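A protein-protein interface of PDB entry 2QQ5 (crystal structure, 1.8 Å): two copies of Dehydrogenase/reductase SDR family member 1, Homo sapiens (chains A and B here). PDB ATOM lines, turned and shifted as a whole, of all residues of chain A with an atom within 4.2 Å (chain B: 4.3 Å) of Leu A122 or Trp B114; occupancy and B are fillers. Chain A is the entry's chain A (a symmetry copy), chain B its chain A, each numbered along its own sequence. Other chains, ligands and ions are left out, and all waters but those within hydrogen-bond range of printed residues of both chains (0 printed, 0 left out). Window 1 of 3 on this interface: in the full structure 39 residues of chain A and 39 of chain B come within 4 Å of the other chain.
Leu A122 touches just one residue of chain B: Trp B114.
Trp B114 touches just these residues of chain A: Leu A122 (3.8 Å), Arg A123 (3.7 Å) and Tyr A126 (3.5 Å).
Printed residues of chain B within 4 Å of Ala A167: Val B163 (3.4 Å).
Of the printed residues of chain A, Met B113 touches Tyr A126 (3.9 Å).
Of the printed residues of chain A, Asp B115 touches Arg A123 (2.8 Å).
Of the printed residues of chain B, Tyr A126 touches Ala B111, Met B113, Trp B114 and Pro B160.
Cys A168 touches none of the printed residues of chain B.
The nearest printed residue of chain A that does not touch Trp B114 is Ala A167 (5.3 Å).
Of the 11 printed residues of chain B, 6 touch a printed residue of chain A.
Of the 12 printed residues of chain A, 4 touch a printed residue of chain B.
Hydrophobic or aromatic side chains of chain A that line the printed part of chain B: Leu A122, Tyr A126 and Ala A167.
Along chain A the printed residues that touch a printed residue of chain B span positions 122 to 167.
Among the printed residues, 8 pairs touch across the chains.
The side-chain carboxylate (OD1) of Asp B115 lies within salt-bridge range of the guanidinium group (NE) of Arg A123, at 2.8 Å.
Among the printed residues, merely in contact across the chains: Leu A122 with Trp B114, Arg A123 with Trp B114, Tyr A126 with Ala B111, Tyr A126 with Met B113, Tyr A126 with Trp B114, Tyr A126 with Pro B160 and Ala A167 with Val B163.
The side-chain amide nitrogen (ND2) of Asn B118 is in hydrogen-bond range of the backbone carbonyl oxygen (O) of Pro B160.
N of Arg A123 lies within hydrogen-bond range of O of Asn A118 (3.4 Å).
OD1 of Asn A119 is in hydrogen-bond range of NH1 of Arg A123, 2.9 Å away.
Positions printed for both chains: 118 and 119.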
ATOM      1  N   ASN A 118      20.958  -2.242 -15.176  1.00  0.00           N
ATOM      2  CA  ASN A 118      21.545  -0.909 -15.079  1.00  0.00           C
ATOM      3  C   ASN A 118      22.597  -0.753 -14.004  1.00  0.00           C
ATOM      4  O   ASN A 118      22.959   0.365 -13.664  1.00  0.00           O
ATOM      5  CB  ASN A 118      20.429   0.131 -14.917  1.00  0.00           C
ATOM      6  CG  ASN A 118      19.582   0.241 -16.171  1.00  0.00           C
ATOM      7  OD1 ASN A 118      20.108   0.115 -17.277  1.00  0.00           O
ATOM      8  ND2 ASN A 118      18.257   0.435 -16.008  1.00  0.00           N
ATOM      9  N   ASN A 119      23.087  -1.871 -13.462  1.00  0.00           N
ATOM     10  CA  ASN A 119      24.261  -1.804 -12.605  1.00  0.00           C
ATOM     11  C   ASN A 119      25.523  -1.900 -13.475  1.00  0.00           C
ATOM     12  O   ASN A 119      26.047  -0.875 -13.896  1.00  0.00           O
ATOM     13  CB  ASN A 119      24.196  -2.798 -11.438  1.00  0.00           C
ATOM     14  CG  ASN A 119      25.134  -2.431 -10.335  1.00  0.00           C
ATOM     15  OD1 ASN A 119      25.974  -1.562 -10.511  1.00  0.00           O
ATOM     16  ND2 ASN A 119      25.000  -3.069  -9.198  1.00  0.00           N
ATOM     17  N   VAL A 120      25.970  -3.107 -13.797  1.00  0.00           N
ATOM     18  CA  VAL A 120      27.064  -3.279 -14.738  1.00  0.00           C
ATOM     19  C   VAL A 120      26.791  -2.509 -16.053  1.00  0.00           C
ATOM     20  O   VAL A 120      27.708  -1.859 -16.597  1.00  0.00           O
ATOM     21  CB  VAL A 120      27.294  -4.784 -15.006  1.00  0.00           C
ATOM     22  CG1 VAL A 120      28.228  -4.972 -16.179  1.00  0.00           C
ATOM     23  CG2 VAL A 120      27.826  -5.463 -13.741  1.00  0.00           C
ATOM     24  N   GLY A 121      25.546  -2.534 -16.534  1.00  0.00           N
ATOM     25  CA  GLY A 121      25.182  -1.926 -17.810  1.00  0.00           C
ATOM     26  C   GLY A 121      24.864  -0.440 -17.855  1.00  0.00           C
ATOM     27  O   GLY A 121      24.415   0.077 -18.887  1.00  0.00           O
ATOM     28  N   LEU A 122      25.070   0.249 -16.749  1.00  0.00           N
ATOM     29  CA  LEU A 122      25.015   1.725 -16.753  1.00  0.00           C
ATOM     30  C   LEU A 122      26.013   2.294 -15.780  1.00  0.00           C
ATOM     31  O   LEU A 122      26.976   2.979 -16.184  1.00  0.00           O
ATOM     32  CB  LEU A 122      23.590   2.238 -16.488  1.00  0.00           C
ATOM     33  CG  LEU A 122      23.442   3.768 -16.451  1.00  0.00           C
ATOM     34  CD1 LEU A 122      23.849   4.379 -17.793  1.00  0.00           C
ATOM     35  CD2 LEU A 122      21.980   4.152 -16.067  1.00  0.00           C
ATOM     36  N   ARG A 123      25.830   1.953 -14.507  1.00  0.00           N
ATOM     37  CA  ARG A 123      26.695   2.400 -13.439  1.00  0.00           C
ATOM     38  C   ARG A 123      28.154   2.007 -13.705  1.00  0.00           C
ATOM     39  O   ARG A 123      29.053   2.841 -13.572  1.00  0.00           O
ATOM     40  CB  ARG A 123      26.173   1.820 -12.131  1.00  0.00           C
ATOM     41  CG  ARG A 123      26.846   2.221 -10.903  1.00  0.00           C
ATOM     42  CD  ARG A 123      25.983   1.817  -9.736  1.00  0.00           C
ATOM     43  NE  ARG A 123      26.746   1.955  -8.524  1.00  0.00           N
ATOM     44  CZ  ARG A 123      27.544   1.014  -8.041  1.00  0.00           C
ATOM     45  NH1 ARG A 123      27.668  -0.169  -8.647  1.00  0.00           N
ATOM     46  NH2 ARG A 123      28.230   1.274  -6.950  1.00  0.00           N
ATOM     47  N   GLY A 124      28.379   0.751 -14.112  1.00  0.00           N
ATOM     48  CA  GLY A 124      29.726   0.268 -14.452  1.00  0.00           C
ATOM     49  C   GLY A 124      30.369   1.035 -15.614  1.00  0.00           C
ATOM     50  O   GLY A 124      31.593   1.275 -15.623  1.00  0.00           O
ATOM     51  N   HIS A 125      29.571   1.386 -16.592  1.00  0.00           N
ATOM     52  CA  HIS A 125      30.046   2.192 -17.724  1.00  0.00           C
ATOM     53  C   HIS A 125      30.577   3.541 -17.225  1.00  0.00           C
ATOM     54  O   HIS A 125      31.612   3.996 -17.689  1.00  0.00           O
ATOM     55  CB  HIS A 125      28.949   2.439 -18.751  1.00  0.00           C
ATOM     56  CG  HIS A 125      28.468   1.211 -19.454  1.00  0.00           C
ATOM     57  ND1 HIS A 125      29.233   0.080 -19.617  1.00  0.00           N
ATOM     58  CD2 HIS A 125      27.285   0.956 -20.058  1.00  0.00           C
ATOM     59  CE1 HIS A 125      28.540  -0.822 -20.294  1.00  0.00           C
ATOM     60  NE2 HIS A 125      27.353  -0.311 -20.568  1.00  0.00           N
ATOM     61  N   TYR A 126      29.877   4.161 -16.276  1.00  0.00           N
ATOM     62  CA  TYR A 126      30.348   5.429 -15.685  1.00  0.00           C
ATOM     63  C   TYR A 126      31.693   5.234 -14.983  1.00  0.00           C
ATOM     64  O   TYR A 126      32.646   5.982 -15.207  1.00  0.00           O
ATOM     65  CB  TYR A 126      29.331   6.073 -14.724  1.00  0.00           C
ATOM     66  CG  TYR A 126      29.783   7.443 -14.240  1.00  0.00           C
ATOM     67  CD1 TYR A 126      29.657   8.556 -15.062  1.00  0.00           C
ATOM     68  CD2 TYR A 126      30.384   7.616 -12.988  1.00  0.00           C
ATOM     69  CE1 TYR A 126      30.063   9.791 -14.657  1.00  0.00           C
ATOM     70  CE2 TYR A 126      30.816   8.882 -12.564  1.00  0.00           C
ATOM     71  CZ  TYR A 126      30.651   9.955 -13.407  1.00  0.00           C
ATOM     72  OH  TYR A 126      31.016  11.223 -13.054  1.00  0.00           O
ATOM     73  N   GLY A 164      17.949   2.655 -19.416  1.00  0.00           N
ATOM     74  CA  GLY A 164      19.378   2.460 -19.450  1.00  0.00           C
ATOM     75  C   GLY A 164      20.004   2.928 -20.747  1.00  0.00           C
ATOM     76  O   GLY A 164      21.091   3.524 -20.749  1.00  0.00           O
ATOM     77  N   ALA A 167      20.076   6.617 -20.932  1.00  0.00           N
ATOM     78  CA  ALA A 167      21.176   7.061 -20.102  1.00  0.00           C
ATOM     79  C   ALA A 167      22.534   6.872 -20.783  1.00  0.00           C
ATOM     80  O   ALA A 167      23.419   7.724 -20.661  1.00  0.00           O
ATOM     81  CB  ALA A 167      21.162   6.345 -18.735  1.00  0.00           C
ATOM     82  N   CYS A 168      22.718   5.743 -21.453  1.00  0.00           N
ATOM     83  CA  CYS A 168      23.981   5.460 -22.170  1.00  0.00           C
ATOM     84  C   CYS A 168      24.249   6.460 -23.304  1.00  0.00           C
ATOM     85  O   CYS A 168      25.391   6.926 -23.492  1.00  0.00           O
ATOM     86  CB  CYS A 168      24.002   4.008 -22.727  1.00  0.00           C
ATOM     87  SG  CYS A 168      24.153   2.723 -21.497  1.00  0.00           S
ATOM     88  N   ALA B 111      34.807   8.578  -8.873  1.00  0.00           N
ATOM     89  CA  ALA B 111      33.912   7.740  -9.650  1.00  0.00           C
ATOM     90  C   ALA B 111      32.604   7.537  -8.895  1.00  0.00           C
ATOM     91  O   ALA B 111      31.530   7.499  -9.496  1.00  0.00           O
ATOM     92  CB  ALA B 111      34.609   6.385  -9.991  1.00  0.00           C
ATOM     93  N   SER B 112      32.681   7.476  -7.561  1.00  0.00           N
ATOM     94  CA  SER B 112      31.527   7.195  -6.722  1.00  0.00           C
ATOM     95  C   SER B 112      30.509   8.354  -6.712  1.00  0.00           C
ATOM     96  O   SER B 112      29.393   8.196  -6.201  1.00  0.00           O
ATOM     97  CB  SER B 112      31.976   6.861  -5.293  1.00  0.00           C
ATOM     98  OG  SER B 112      32.641   7.986  -4.718  1.00  0.00           O
ATOM     99  N   MET B 113      30.868   9.507  -7.295  1.00  0.00           N
ATOM    100  CA  MET B 113      29.921  10.615  -7.419  1.00  0.00           C
ATOM    101  C   MET B 113      28.631  10.190  -8.146  1.00  0.00           C
ATOM    102  O   MET B 113      27.558  10.731  -7.887  1.00  0.00           O
ATOM    103  CB  MET B 113      30.558  11.845  -8.105  1.00  0.00           C
ATOM    104  CG  MET B 113      29.685  13.103  -8.012  1.00  0.00           C
ATOM    105  SD  MET B 113      30.434  14.568  -8.772  1.00  0.00           S
ATOM    106  CE  MET B 113      30.509  14.101 -10.479  1.00  0.00           C
ATOM    107  N   TRP B 114      28.727   9.207  -9.036  1.00  0.00           N
ATOM    108  CA  TRP B 114      27.549   8.645  -9.666  1.00  0.00           C
ATOM    109  C   TRP B 114      26.531   8.271  -8.612  1.00  0.00           C
ATOM    110  O   TRP B 114      25.350   8.620  -8.728  1.00  0.00           O
ATOM    111  CB  TRP B 114      27.918   7.418 -10.502  1.00  0.00           C
ATOM    112  CG  TRP B 114      26.724   6.747 -11.065  1.00  0.00           C
ATOM    113  CD1 TRP B 114      25.960   5.805 -10.448  1.00  0.00           C
ATOM    114  CD2 TRP B 114      26.114   6.997 -12.329  1.00  0.00           C
ATOM    115  NE1 TRP B 114      24.924   5.433 -11.246  1.00  0.00           N
ATOM    116  CE2 TRP B 114      24.982   6.142 -12.413  1.00  0.00           C
ATOM    117  CE3 TRP B 114      26.427   7.827 -13.420  1.00  0.00           C
ATOM    118  CZ2 TRP B 114      24.163   6.084 -13.541  1.00  0.00           C
ATOM    119  CZ3 TRP B 114      25.592   7.787 -14.533  1.00  0.00           C
ATOM    120  CH2 TRP B 114      24.463   6.923 -14.583  1.00  0.00           C
ATOM    121  N   ASP B 115      26.978   7.593  -7.553  1.00  0.00           N
ATOM    122  CA  ASP B 115      26.021   7.090  -6.560  1.00  0.00           C
ATOM    123  C   ASP B 115      25.391   8.190  -5.695  1.00  0.00           C
ATOM    124  O   ASP B 115      24.305   7.984  -5.123  1.00  0.00           O
ATOM    125  CB  ASP B 115      26.664   6.032  -5.664  1.00  0.00           C
ATOM    126  CG  ASP B 115      26.931   4.722  -6.411  1.00  0.00           C
ATOM    127  OD1 ASP B 115      26.159   4.368  -7.334  1.00  0.00           O
ATOM    128  OD2 ASP B 115      27.929   4.062  -6.070  1.00  0.00           O
ATOM    129  N   ASP B 116      26.058   9.337  -5.613  1.00  0.00           N
ATOM    130  CA  ASP B 116      25.534  10.474  -4.835  1.00  0.00           C
ATOM    131  C   ASP B 116      24.359  11.115  -5.544  1.00  0.00           C
ATOM    132  O   ASP B 116      23.531  11.762  -4.900  1.00  0.00           O
ATOM    133  CB  ASP B 116      26.604  11.539  -4.622  1.00  0.00           C
ATOM    134  CG  ASP B 116      27.756  11.049  -3.770  1.00  0.00           C
ATOM    135  OD1 ASP B 116      27.547  10.192  -2.899  1.00  0.00           O
ATOM    136  OD2 ASP B 116      28.868  11.530  -3.985  1.00  0.00           O
ATOM    137  N   ILE B 117      24.304  10.944  -6.870  1.00  0.00           N
ATOM    138  CA  ILE B 117      23.328  11.605  -7.727  1.00  0.00           C
ATOM    139  C   ILE B 117      22.276  10.629  -8.300  1.00  0.00           C
ATOM    140  O   ILE B 117      21.095  10.973  -8.380  1.00  0.00           O
ATOM    141  CB  ILE B 117      24.075  12.322  -8.858  1.00  0.00           C
ATOM    142  CG1 ILE B 117      24.953  13.420  -8.258  1.00  0.00           C
ATOM    143  CG2 ILE B 117      23.097  12.903  -9.926  1.00  0.00           C
ATOM    144  CD1 ILE B 117      25.979  13.989  -9.204  1.00  0.00           C
ATOM    145  N   ASN B 118      22.702   9.418  -8.674  1.00  0.00           N
ATOM    146  CA  ASN B 118      21.863   8.483  -9.417  1.00  0.00           C
ATOM    147  C   ASN B 118      21.520   7.210  -8.677  1.00  0.00           C
ATOM    148  O   ASN B 118      21.052   6.258  -9.289  1.00  0.00           O
ATOM    149  CB  ASN B 118      22.512   8.179 -10.773  1.00  0.00           C
ATOM    150  CG  ASN B 118      22.515   9.398 -11.677  1.00  0.00           C
ATOM    151  OD1 ASN B 118      21.569  10.186 -11.644  1.00  0.00           O
ATOM    152  ND2 ASN B 118      23.598   9.585 -12.459  1.00  0.00           N
ATOM    153  N   ASN B 119      21.755   7.183  -7.363  1.00  0.00           N
ATOM    154  CA  ASN B 119      21.232   6.092  -6.556  1.00  0.00           C
ATOM    155  C   ASN B 119      19.808   6.444  -6.101  1.00  0.00           C
ATOM    156  O   ASN B 119      18.852   6.099  -6.786  1.00  0.00           O
ATOM    157  CB  ASN B 119      22.192   5.675  -5.434  1.00  0.00           C
ATOM    158  CG  ASN B 119      21.888   4.309  -4.914  1.00  0.00           C
ATOM    159  OD1 ASN B 119      20.852   3.748  -5.238  1.00  0.00           O
ATOM    160  ND2 ASN B 119      22.777   3.758  -4.123  1.00  0.00           N
ATOM    161  N   PRO B 160      27.010  13.082 -14.398  1.00  0.00           N
ATOM    162  CA  PRO B 160      25.971  12.258 -13.771  1.00  0.00           C
ATOM    163  C   PRO B 160      24.624  12.955 -13.632  1.00  0.00           C
ATOM    164  O   PRO B 160      23.593  12.287 -13.723  1.00  0.00           O
ATOM    165  CB  PRO B 160      26.545  11.938 -12.398  1.00  0.00           C
ATOM    166  CG  PRO B 160      27.992  12.118 -12.531  1.00  0.00           C
ATOM    167  CD  PRO B 160      28.198  13.226 -13.531  1.00  0.00           C
ATOM    168  N   VAL B 163      22.947  12.785 -17.225  1.00  0.00           N
ATOM    169  CA  VAL B 163      22.632  11.409 -17.545  1.00  0.00           C
ATOM    170  C   VAL B 163      21.413  10.963 -16.733  1.00  0.00           C
ATOM    171  O   VAL B 163      20.488  10.340 -17.275  1.00  0.00           O
ATOM    172  CB  VAL B 163      23.827  10.483 -17.312  1.00  0.00           C
ATOM    173  CG1 VAL B 163      23.408   8.992 -17.477  1.00  0.00           C
ATOM    174  CG2 VAL B 163      25.032  10.843 -18.281  1.00  0.00           C
